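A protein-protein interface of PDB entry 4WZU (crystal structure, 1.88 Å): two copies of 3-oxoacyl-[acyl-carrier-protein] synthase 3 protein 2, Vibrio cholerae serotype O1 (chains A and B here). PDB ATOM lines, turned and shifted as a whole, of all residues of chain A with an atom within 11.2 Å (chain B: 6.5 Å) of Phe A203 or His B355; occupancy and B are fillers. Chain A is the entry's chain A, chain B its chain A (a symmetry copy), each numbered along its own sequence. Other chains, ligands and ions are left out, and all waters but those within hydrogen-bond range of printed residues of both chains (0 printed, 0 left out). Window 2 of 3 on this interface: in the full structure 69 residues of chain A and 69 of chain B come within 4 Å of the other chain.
Phe B145 touches Thr A198.
CE1 of Phe B145 touches O of Met A200, 3.6 Å away.
Phe A203 touches Tyr B209 (CE1 to CE1, 3.7 Å).
CA of Ala B352 touches CE2 of Phe A203, 3.8 Å away.
CB of Phe A203 touches CD2 of His B355 (3.4 Å).
Cys B356 touches Phe A203 (SG to CZ, 3.8 Å).
Of the 17 printed residues of chain B, 7 touch a printed residue of chain A.
Printed residues of chain B that touch a printed residue of chain A: Phe B145, Leu B147, Gly B208, Tyr B209, Ala B352, His B355 and Cys B356.
Hydrophobic or aromatic side chains of chain B that line the printed part of chain A: Phe B145, Tyr B209, Ala B352 and His B355.
Among the printed residues, no Asp or Glu carboxylate lies within 4 Å of a Lys or Arg side-chain nitrogen of the other chain.
O of Phe B145 lies within hydrogen-bond range of NH1 of Arg A202 (2.9 Å).
The guanidinium group (NH1) of Arg A202 is in hydrogen-bond range of the backbone carbonyl oxygen (O) of Leu B147.
The backbone carbonyl oxygen (O) of Gly B208 is in hydrogen-bond range of the guanidinium group (NE) of Arg A202 (2.8 Å).
The backbone NH (N) of Gly A197 sits at hydrogen-bond distance from the side-chain sulfur (SD) of Met A200 (3.7 Å).
The side-chain carboxylate of Asp A201 sits at hydrogen-bond distance from the backbone NH of Phe A203, 3.1 Å away.
The side-chain amide nitrogen (ND2) of Asn A207 is in hydrogen-bond range of the backbone carbonyl oxygen (O) of Arg A202 (3.5 Å).
The backbone NH of Trp B149 sits at hydrogen-bond distance from the side-chain sulfur of Cys B356, at 3.8 Å.
The side-chain sulfur (SG) of Cys B356 is in hydrogen-bond range of the backbone carbonyl oxygen (O) of Ala B352.
Of the printed residues of chain B, Phe A203 touches Tyr B209, Ala B352, His B355 and Cys B356.
His B355 touches just one residue of chain A: Phe A203.
Gly B208 touches just one residue of chain A: Arg A202 (2.8 Å).
Lys B351 touches none of the printed residues of chain A.
Printed residues of chain A within 4 Å of Ala B352: Phe A203 (3.8 Å).
No residue of chain A comes within 4 Å of Glu B354.
Cys B356 touches just one residue of chain A: Phe A203 (3.8 Å).
No residue of chain A comes within 4 Å of Lys B357.
No residue of chain A comes within 4 Å of Arg B358.
No residue of chain A comes within 4 Å of His B359.
Of the printed residues of chain B, Met A200 touches Phe B145 (3.6 Å).
Of the printed residues of chain A, Phe B145 touches Thr A198, Met A200 and Arg A202.
Of the printed residues of chain A, Tyr B209 touches Phe A203 (3.7 Å).
Of the printed residues of chain A, Leu B147 touches Arg A202.
The nearest residue of chain B that does not touch Phe A203 is Gly B208 (4.04 Å).
The nearest printed residue of chain A that does not touch Phe B145 is Gly A197 (4.1 Å).
Positions printed for both chains: 205, 208 and 209.
Of the 9 pairs that touch across the chains among the printed residues, none has its exchanged pair printed and touching as well.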
ATOM      1  N   LYS A 195      29.678 -28.530  -5.667  1.00  0.00           N
ATOM      2  CA  LYS A 195      29.595 -28.453  -7.118  1.00  0.00           C
ATOM      3  C   LYS A 195      29.424 -29.800  -7.835  1.00  0.00           C
ATOM      4  O   LYS A 195      29.871 -29.987  -8.982  1.00  0.00           O
ATOM      5  CB  LYS A 195      30.816 -27.703  -7.651  1.00  0.00           C
ATOM      6  CG  LYS A 195      30.511 -26.254  -7.962  1.00  0.00           C
ATOM      7  CD  LYS A 195      30.203 -25.423  -6.731  1.00  0.00           C
ATOM      8  CE  LYS A 195      30.072 -23.942  -7.098  1.00  0.00           C
ATOM      9  NZ  LYS A 195      28.759 -23.652  -7.747  1.00  0.00           N
ATOM     10  N   GLY A 197      25.789 -31.634  -8.509  1.00  0.00           N
ATOM     11  CA  GLY A 197      24.348 -31.432  -8.370  1.00  0.00           C
ATOM     12  C   GLY A 197      23.992 -30.324  -9.345  1.00  0.00           C
ATOM     13  O   GLY A 197      24.823 -29.951 -10.186  1.00  0.00           O
ATOM     14  N   THR A 198      22.794 -29.765  -9.223  1.00  0.00           N
ATOM     15  CA  THR A 198      22.337 -28.737 -10.180  1.00  0.00           C
ATOM     16  C   THR A 198      22.975 -27.357 -10.016  1.00  0.00           C
ATOM     17  O   THR A 198      22.687 -26.455 -10.814  1.00  0.00           O
ATOM     18  CB  THR A 198      20.798 -28.583 -10.136  1.00  0.00           C
ATOM     19  OG1 THR A 198      20.400 -28.154  -8.841  1.00  0.00           O
ATOM     20  CG2 THR A 198      20.139 -29.890 -10.447  1.00  0.00           C
ATOM     21  N   ALA A 199      23.840 -27.198  -9.003  1.00  0.00           N
ATOM     22  CA  ALA A 199      24.670 -26.000  -8.860  1.00  0.00           C
ATOM     23  C   ALA A 199      25.870 -26.050  -9.800  1.00  0.00           C
ATOM     24  O   ALA A 199      26.519 -25.035  -9.985  1.00  0.00           O
ATOM     25  CB  ALA A 199      25.153 -25.820  -7.422  1.00  0.00           C
ATOM     26  N   MET A 200      26.177 -27.214 -10.373  1.00  0.00           N
ATOM     27  CA  MET A 200      27.322 -27.346 -11.272  1.00  0.00           C
ATOM     28  C   MET A 200      27.002 -26.824 -12.680  1.00  0.00           C
ATOM     29  O   MET A 200      25.835 -26.753 -13.095  1.00  0.00           O
ATOM     30  CB  MET A 200      27.790 -28.811 -11.327  1.00  0.00           C
ATOM     31  CG  MET A 200      27.041 -29.714 -12.306  1.00  0.00           C
ATOM     32  SD  MET A 200      27.234 -31.477 -11.927  1.00  0.00           S
ATOM     33  CE  MET A 200      28.989 -31.717 -12.242  1.00  0.00           C
ATOM     34  N   ASP A 201      28.053 -26.467 -13.402  1.00  0.00           N
ATOM     35  CA  ASP A 201      27.949 -26.018 -14.790  1.00  0.00           C
ATOM     36  C   ASP A 201      27.963 -27.260 -15.667  1.00  0.00           C
ATOM     37  O   ASP A 201      29.001 -27.888 -15.876  1.00  0.00           O
ATOM     38  CB  ASP A 201      29.107 -25.080 -15.150  1.00  0.00           C
ATOM     39  CG  ASP A 201      28.995 -24.496 -16.566  1.00  0.00           C
ATOM     40  OD1 ASP A 201      28.204 -24.976 -17.416  1.00  0.00           O
ATOM     41  OD2 ASP A 201      29.738 -23.541 -16.832  1.00  0.00           O
ATOM     42  N   ARG A 202      26.788 -27.601 -16.167  1.00  0.00           N
ATOM     43  CA  ARG A 202      26.583 -28.778 -16.985  1.00  0.00           C
ATOM     44  C   ARG A 202      27.515 -28.859 -18.192  1.00  0.00           C
ATOM     45  O   ARG A 202      27.921 -29.952 -18.586  1.00  0.00           O
ATOM     46  CB  ARG A 202      25.127 -28.778 -17.471  1.00  0.00           C
ATOM     47  CG  ARG A 202      24.716 -29.975 -18.304  1.00  0.00           C
ATOM     48  CD  ARG A 202      23.206 -29.998 -18.505  1.00  0.00           C
ATOM     49  NE  ARG A 202      22.860 -30.811 -19.664  1.00  0.00           N
ATOM     50  CZ  ARG A 202      21.662 -30.850 -20.248  1.00  0.00           C
ATOM     51  NH1 ARG A 202      20.644 -30.139 -19.782  1.00  0.00           N
ATOM     52  NH2 ARG A 202      21.492 -31.608 -21.324  1.00  0.00           N
ATOM     53  N   PHE A 203      27.834 -27.719 -18.795  1.00  0.00           N
ATOM     54  CA  PHE A 203      28.552 -27.737 -20.083  1.00  0.00           C
ATOM     55  C   PHE A 203      30.020 -27.326 -19.984  1.00  0.00           C
ATOM     56  O   PHE A 203      30.706 -27.222 -20.996  1.00  0.00           O
ATOM     57  CB  PHE A 203      27.785 -26.898 -21.110  1.00  0.00           C
ATOM     58  CG  PHE A 203      26.404 -27.422 -21.395  1.00  0.00           C
ATOM     59  CD1 PHE A 203      26.230 -28.633 -22.066  1.00  0.00           C
ATOM     60  CD2 PHE A 203      25.273 -26.722 -20.986  1.00  0.00           C
ATOM     61  CE1 PHE A 203      24.957 -29.131 -22.322  1.00  0.00           C
ATOM     62  CE2 PHE A 203      24.000 -27.212 -21.245  1.00  0.00           C
ATOM     63  CZ  PHE A 203      23.841 -28.417 -21.915  1.00  0.00           C
ATOM     64  N   ASP A 204      30.501 -27.108 -18.765  1.00  0.00           N
ATOM     65  CA  ASP A 204      31.917 -26.835 -18.523  1.00  0.00           C
ATOM     66  C   ASP A 204      32.701 -28.151 -18.467  1.00  0.00           C
ATOM     67  O   ASP A 204      32.502 -28.977 -17.566  1.00  0.00           O
ATOM     68  CB  ASP A 204      32.105 -26.059 -17.210  1.00  0.00           C
ATOM     69  CG  ASP A 204      33.563 -25.781 -16.891  1.00  0.00           C
ATOM     70  OD1 ASP A 204      34.460 -26.106 -17.702  1.00  0.00           O
ATOM     71  OD2 ASP A 204      33.823 -25.206 -15.825  1.00  0.00           O
ATOM     72  N   ALA A 205      33.621 -28.319 -19.408  1.00  0.00           N
ATOM     73  CA  ALA A 205      34.456 -29.518 -19.469  1.00  0.00           C
ATOM     74  C   ALA A 205      35.362 -29.783 -18.247  1.00  0.00           C
ATOM     75  O   ALA A 205      35.836 -30.905 -18.090  1.00  0.00           O
ATOM     76  CB  ALA A 205      35.287 -29.505 -20.729  1.00  0.00           C
ATOM     77  N   ASP A 206      35.601 -28.784 -17.390  1.00  0.00           N
ATOM     78  CA  ASP A 206      36.309 -29.001 -16.103  1.00  0.00           C
ATOM     79  C   ASP A 206      35.394 -29.259 -14.890  1.00  0.00           C
ATOM     80  O   ASP A 206      35.844 -29.184 -13.738  1.00  0.00           O
ATOM     81  CB  ASP A 206      37.208 -27.804 -15.790  1.00  0.00           C
ATOM     82  CG  ASP A 206      38.324 -27.639 -16.796  1.00  0.00           C
ATOM     83  OD1 ASP A 206      38.459 -28.497 -17.697  1.00  0.00           O
ATOM     84  OD2 ASP A 206      39.071 -26.643 -16.687  1.00  0.00           O
ATOM     85  N   ASN A 207      34.127 -29.579 -15.135  1.00  0.00           N
ATOM     86  CA  ASN A 207      33.155 -29.708 -14.027  1.00  0.00           C
ATOM     87  C   ASN A 207      33.300 -30.986 -13.165  1.00  0.00           C
ATOM     88  O   ASN A 207      32.695 -31.098 -12.090  1.00  0.00           O
ATOM     89  CB  ASN A 207      31.708 -29.501 -14.537  1.00  0.00           C
ATOM     90  CG  ASN A 207      31.182 -30.653 -15.393  1.00  0.00           C
ATOM     91  OD1 ASN A 207      31.862 -31.649 -15.629  1.00  0.00           O
ATOM     92  ND2 ASN A 207      29.930 -30.521 -15.835  1.00  0.00           N
ATOM     93  N   GLY A 208      34.084 -31.946 -13.648  1.00  0.00           N
ATOM     94  CA  GLY A 208      34.443 -33.131 -12.880  1.00  0.00           C
ATOM     95  C   GLY A 208      35.449 -32.861 -11.762  1.00  0.00           C
ATOM     96  O   GLY A 208      35.556 -33.660 -10.833  1.00  0.00           O
ATOM     97  N   TYR A 209      36.167 -31.740 -11.826  1.00  0.00           N
ATOM     98  CA  TYR A 209      37.238 -31.445 -10.859  1.00  0.00           C
ATOM     99  C   TYR A 209      36.734 -30.580  -9.711  1.00  0.00           C
ATOM    100  O   TYR A 209      37.210 -29.478  -9.492  1.00  0.00           O
ATOM    101  CB  TYR A 209      38.434 -30.793 -11.581  1.00  0.00           C
ATOM    102  CG  TYR A 209      38.912 -31.652 -12.729  1.00  0.00           C
ATOM    103  CD1 TYR A 209      39.745 -32.744 -12.503  1.00  0.00           C
ATOM    104  CD2 TYR A 209      38.474 -31.419 -14.033  1.00  0.00           C
ATOM    105  CE1 TYR A 209      40.165 -33.560 -13.551  1.00  0.00           C
ATOM    106  CE2 TYR A 209      38.890 -32.226 -15.092  1.00  0.00           C
ATOM    107  CZ  TYR A 209      39.736 -33.297 -14.846  1.00  0.00           C
ATOM    108  OH  TYR A 209      40.141 -34.110 -15.879  1.00  0.00           O
ATOM    109  N   PHE B 145      17.526 -27.279 -15.442  1.00  0.00           N
ATOM    110  CA  PHE B 145      18.882 -27.836 -15.446  1.00  0.00           C
ATOM    111  C   PHE B 145      19.026 -29.007 -16.425  1.00  0.00           C
ATOM    112  O   PHE B 145      20.043 -29.149 -17.082  1.00  0.00           O
ATOM    113  CB  PHE B 145      19.264 -28.309 -14.053  1.00  0.00           C
ATOM    114  CG  PHE B 145      20.615 -28.984 -13.991  1.00  0.00           C
ATOM    115  CD1 PHE B 145      21.792 -28.230 -14.051  1.00  0.00           C
ATOM    116  CD2 PHE B 145      20.713 -30.363 -13.917  1.00  0.00           C
ATOM    117  CE1 PHE B 145      23.031 -28.852 -14.000  1.00  0.00           C
ATOM    118  CE2 PHE B 145      21.938 -30.989 -13.874  1.00  0.00           C
ATOM    119  CZ  PHE B 145      23.103 -30.233 -13.903  1.00  0.00           C
ATOM    120  N   LEU B 147      17.128 -30.201 -19.123  1.00  0.00           N
ATOM    121  CA  LEU B 147      16.427 -30.316 -20.393  1.00  0.00           C
ATOM    122  C   LEU B 147      17.378 -30.282 -21.576  1.00  0.00           C
ATOM    123  O   LEU B 147      18.427 -29.653 -21.536  1.00  0.00           O
ATOM    124  CB  LEU B 147      15.380 -29.205 -20.527  1.00  0.00           C
ATOM    125  CG  LEU B 147      14.348 -29.221 -19.401  1.00  0.00           C
ATOM    126  CD1 LEU B 147      13.280 -28.163 -19.601  1.00  0.00           C
ATOM    127  CD2 LEU B 147      13.708 -30.594 -19.298  1.00  0.00           C
ATOM    128  N   TRP B 149      17.494 -28.956 -25.071  1.00  0.00           N
ATOM    129  CA  TRP B 149      16.782 -27.921 -25.799  1.00  0.00           C
ATOM    130  C   TRP B 149      16.629 -28.213 -27.291  1.00  0.00           C
ATOM    131  O   TRP B 149      16.093 -27.389 -28.007  1.00  0.00           O
ATOM    132  CB  TRP B 149      17.457 -26.578 -25.565  1.00  0.00           C
ATOM    133  CG  TRP B 149      17.457 -26.248 -24.118  1.00  0.00           C
ATOM    134  CD1 TRP B 149      18.531 -26.238 -23.279  1.00  0.00           C
ATOM    135  CD2 TRP B 149      16.313 -25.931 -23.322  1.00  0.00           C
ATOM    136  NE1 TRP B 149      18.127 -25.900 -22.003  1.00  0.00           N
ATOM    137  CE2 TRP B 149      16.770 -25.711 -22.004  1.00  0.00           C
ATOM    138  CE3 TRP B 149      14.946 -25.805 -23.595  1.00  0.00           C
ATOM    139  CZ2 TRP B 149      15.906 -25.368 -20.958  1.00  0.00           C
ATOM    140  CZ3 TRP B 149      14.087 -25.458 -22.567  1.00  0.00           C
ATOM    141  CH2 TRP B 149      14.571 -25.245 -21.257  1.00  0.00           C
ATOM    142  N   ALA B 205      34.101 -35.444 -21.200  1.00  0.00           N
ATOM    143  CA  ALA B 205      33.689 -34.099 -21.603  1.00  0.00           C
ATOM    144  C   ALA B 205      32.330 -33.991 -22.328  1.00  0.00           C
ATOM    145  O   ALA B 205      31.785 -32.893 -22.407  1.00  0.00           O
ATOM    146  CB  ALA B 205      34.768 -33.457 -22.438  1.00  0.00           C
ATOM    147  N   GLY B 208      27.520 -33.916 -20.251  1.00  0.00           N
ATOM    148  CA  GLY B 208      26.394 -32.995 -20.178  1.00  0.00           C
ATOM    149  C   GLY B 208      25.278 -33.303 -21.175  1.00  0.00           C
ATOM    150  O   GLY B 208      24.148 -32.854 -20.983  1.00  0.00           O
ATOM    151  N   TYR B 209      25.571 -34.077 -22.220  1.00  0.00           N
ATOM    152  CA  TYR B 209      24.597 -34.338 -23.293  1.00  0.00           C
ATOM    153  C   TYR B 209      23.837 -35.637 -23.055  1.00  0.00           C
ATOM    154  O   TYR B 209      23.890 -36.557 -23.854  1.00  0.00           O
ATOM    155  CB  TYR B 209      25.306 -34.336 -24.661  1.00  0.00           C
ATOM    156  CG  TYR B 209      26.071 -33.051 -24.876  1.00  0.00           C
ATOM    157  CD1 TYR B 209      25.420 -31.896 -25.301  1.00  0.00           C
ATOM    158  CD2 TYR B 209      27.434 -32.967 -24.585  1.00  0.00           C
ATOM    159  CE1 TYR B 209      26.112 -30.699 -25.472  1.00  0.00           C
ATOM    160  CE2 TYR B 209      28.139 -31.775 -24.756  1.00  0.00           C
ATOM    161  CZ  TYR B 209      27.473 -30.643 -25.199  1.00  0.00           C
ATOM    162  OH  TYR B 209      28.153 -29.456 -25.355  1.00  0.00           O
ATOM    163  N   SER B 350      20.106 -19.077 -23.115  1.00  0.00           N
ATOM    164  CA  SER B 350      20.997 -18.869 -24.258  1.00  0.00           C
ATOM    165  C   SER B 350      22.178 -19.847 -24.400  1.00  0.00           C
ATOM    166  O   SER B 350      22.344 -20.483 -25.452  1.00  0.00           O
ATOM    167  CB  SER B 350      21.533 -17.435 -24.248  1.00  0.00           C
ATOM    168  OG  SER B 350      22.043 -17.110 -25.526  1.00  0.00           O
ATOM    169  N   LYS B 351      23.004 -19.916 -23.361  1.00  0.00           N
ATOM    170  CA  LYS B 351      24.193 -20.779 -23.330  1.00  0.00           C
ATOM    171  C   LYS B 351      23.837 -22.251 -23.502  1.00  0.00           C
ATOM    172  O   LYS B 351      24.386 -22.917 -24.372  1.00  0.00           O
ATOM    173  CB  LYS B 351      24.956 -20.586 -22.021  1.00  0.00           C
ATOM    174  N   ALA B 352      22.910 -22.748 -22.683  1.00  0.00           N
ATOM    175  CA  ALA B 352      22.451 -24.136 -22.790  1.00  0.00           C
ATOM    176  C   ALA B 352      21.869 -24.498 -24.170  1.00  0.00           C
ATOM    177  O   ALA B 352      22.132 -25.579 -24.693  1.00  0.00           O
ATOM    178  CB  ALA B 352      21.440 -24.449 -21.684  1.00  0.00           C
ATOM    179  N   ILE B 353      21.092 -23.593 -24.758  1.00  0.00           N
ATOM    180  CA  ILE B 353      20.467 -23.838 -26.051  1.00  0.00           C
ATOM    181  C   ILE B 353      21.556 -23.980 -27.128  1.00  0.00           C
ATOM    182  O   ILE B 353      21.493 -24.866 -27.979  1.00  0.00           O
ATOM    183  CB  ILE B 353      19.480 -22.704 -26.431  1.00  0.00           C
ATOM    184  CG1 ILE B 353      18.311 -22.638 -25.436  1.00  0.00           C
ATOM    185  CG2 ILE B 353      18.940 -22.902 -27.852  1.00  0.00           C
ATOM    186  CD1 ILE B 353      17.458 -21.388 -25.582  1.00  0.00           C
ATOM    187  N   GLU B 354      22.554 -23.102 -27.082  1.00  0.00           N
ATOM    188  CA  GLU B 354      23.680 -23.146 -28.027  1.00  0.00           C
ATOM    189  C   GLU B 354      24.487 -24.443 -27.886  1.00  0.00           C
ATOM    190  O   GLU B 354      24.837 -25.057 -28.888  1.00  0.00           O
ATOM    191  CB  GLU B 354      24.593 -21.927 -27.836  1.00  0.00           C
ATOM    192  N   HIS B 355      24.765 -24.870 -26.652  1.00  0.00           N
ATOM    193  CA  HIS B 355      25.522 -26.104 -26.433  1.00  0.00           C
ATOM    194  C   HIS B 355      24.780 -27.312 -26.961  1.00  0.00           C
ATOM    195  O   HIS B 355      25.367 -28.164 -27.622  1.00  0.00           O
ATOM    196  CB  HIS B 355      25.837 -26.325 -24.958  1.00  0.00           C
ATOM    197  CG  HIS B 355      26.886 -25.414 -24.422  1.00  0.00           C
ATOM    198  ND1 HIS B 355      28.174 -25.402 -24.903  1.00  0.00           N
ATOM    199  CD2 HIS B 355      26.853 -24.513 -23.413  1.00  0.00           C
ATOM    200  CE1 HIS B 355      28.883 -24.506 -24.244  1.00  0.00           C
ATOM    201  NE2 HIS B 355      28.104 -23.952 -23.335  1.00  0.00           N
ATOM    202  N   CYS B 356      23.489 -27.400 -26.646  1.00  0.00           N
ATOM    203  CA  CYS B 356      22.676 -28.528 -27.102  1.00  0.00           C
ATOM    204  C   CYS B 356      22.616 -28.559 -28.636  1.00  0.00           C
ATOM    205  O   CYS B 356      22.836 -29.609 -29.240  1.00  0.00           O
ATOM    206  CB  CYS B 356      21.271 -28.484 -26.483  1.00  0.00           C
ATOM    207  SG  CYS B 356      21.265 -28.730 -24.688  1.00  0.00           S
ATOM    208  N   LYS B 357      22.348 -27.404 -29.249  1.00  0.00           N
ATOM    209  CA  LYS B 357      22.253 -27.299 -30.708  1.00  0.00           C
ATOM    210  C   LYS B 357      23.585 -27.609 -31.370  1.00  0.00           C
ATOM    211  O   LYS B 357      23.618 -28.276 -32.406  1.00  0.00           O
ATOM    212  CB  LYS B 357      21.786 -25.899 -31.136  1.00  0.00           C
ATOM    213  N   ARG B 358      24.679 -27.122 -30.784  1.00  0.00           N
ATOM    214  CA  ARG B 358      26.024 -27.348 -31.343  1.00  0.00           C
ATOM    215  C   ARG B 358      26.406 -28.834 -31.347  1.00  0.00           C
ATOM    216  O   ARG B 358      27.140 -29.285 -32.215  1.00  0.00           O
ATOM    217  CB  ARG B 358      27.084 -26.525 -30.590  1.00  0.00           C
ATOM    218  N   HIS B 359      25.882 -29.598 -30.392  1.00  0.00           N
ATOM    219  CA  HIS B 359      26.248 -31.010 -30.242  1.00  0.00           C
ATOM    220  C   HIS B 359      25.521 -32.002 -31.173  1.00  0.00           C
ATOM    221  O   HIS B 359      26.046 -33.086 -31.435  1.00  0.00           O
ATOM    222  CB  HIS B 359      26.039 -31.447 -28.781  1.00  0.00           C
ATOM    223  CG  HIS B 359      26.436 -32.867 -28.521  1.00  0.00           C
ATOM    224  ND1 HIS B 359      25.516 -33.888 -28.405  1.00  0.00           N
ATOM    225  CD2 HIS B 359      27.655 -33.441 -28.388  1.00  0.00           C
ATOM    226  CE1 HIS B 359      26.151 -35.027 -28.195  1.00  0.00           C
ATOM    227  NE2 HIS B 359      27.450 -34.783 -28.183  1.00  0.00           N
ATOM    228  N   GLN B 360      24.324 -31.652 -31.653  1.00  0.00           N
ATOM    229  CA  GLN B 360      23.503 -32.582 -32.465  1.00  0.00           C
ATOM    230  C   GLN B 360      24.335 -33.415 -33.443  1.00  0.00           C
ATOM    231  O   GLN B 360      25.069 -32.863 -34.264  1.00  0.00           O
ATOM    232  CB  GLN B 360      22.438 -31.815 -33.256  1.00  0.00           C
ATOM    233  CG  GLN B 360      21.252 -31.344 -32.430  1.00  0.00           C
ATOM    234  CD  GLN B 360      20.491 -30.199 -33.091  1.00  0.00           C
ATOM    235  OE1 GLN B 360      21.090 -29.217 -33.542  1.00  0.00           O
ATOM    236  NE2 GLN B 360      19.165 -30.309 -33.136  1.00  0.00           N
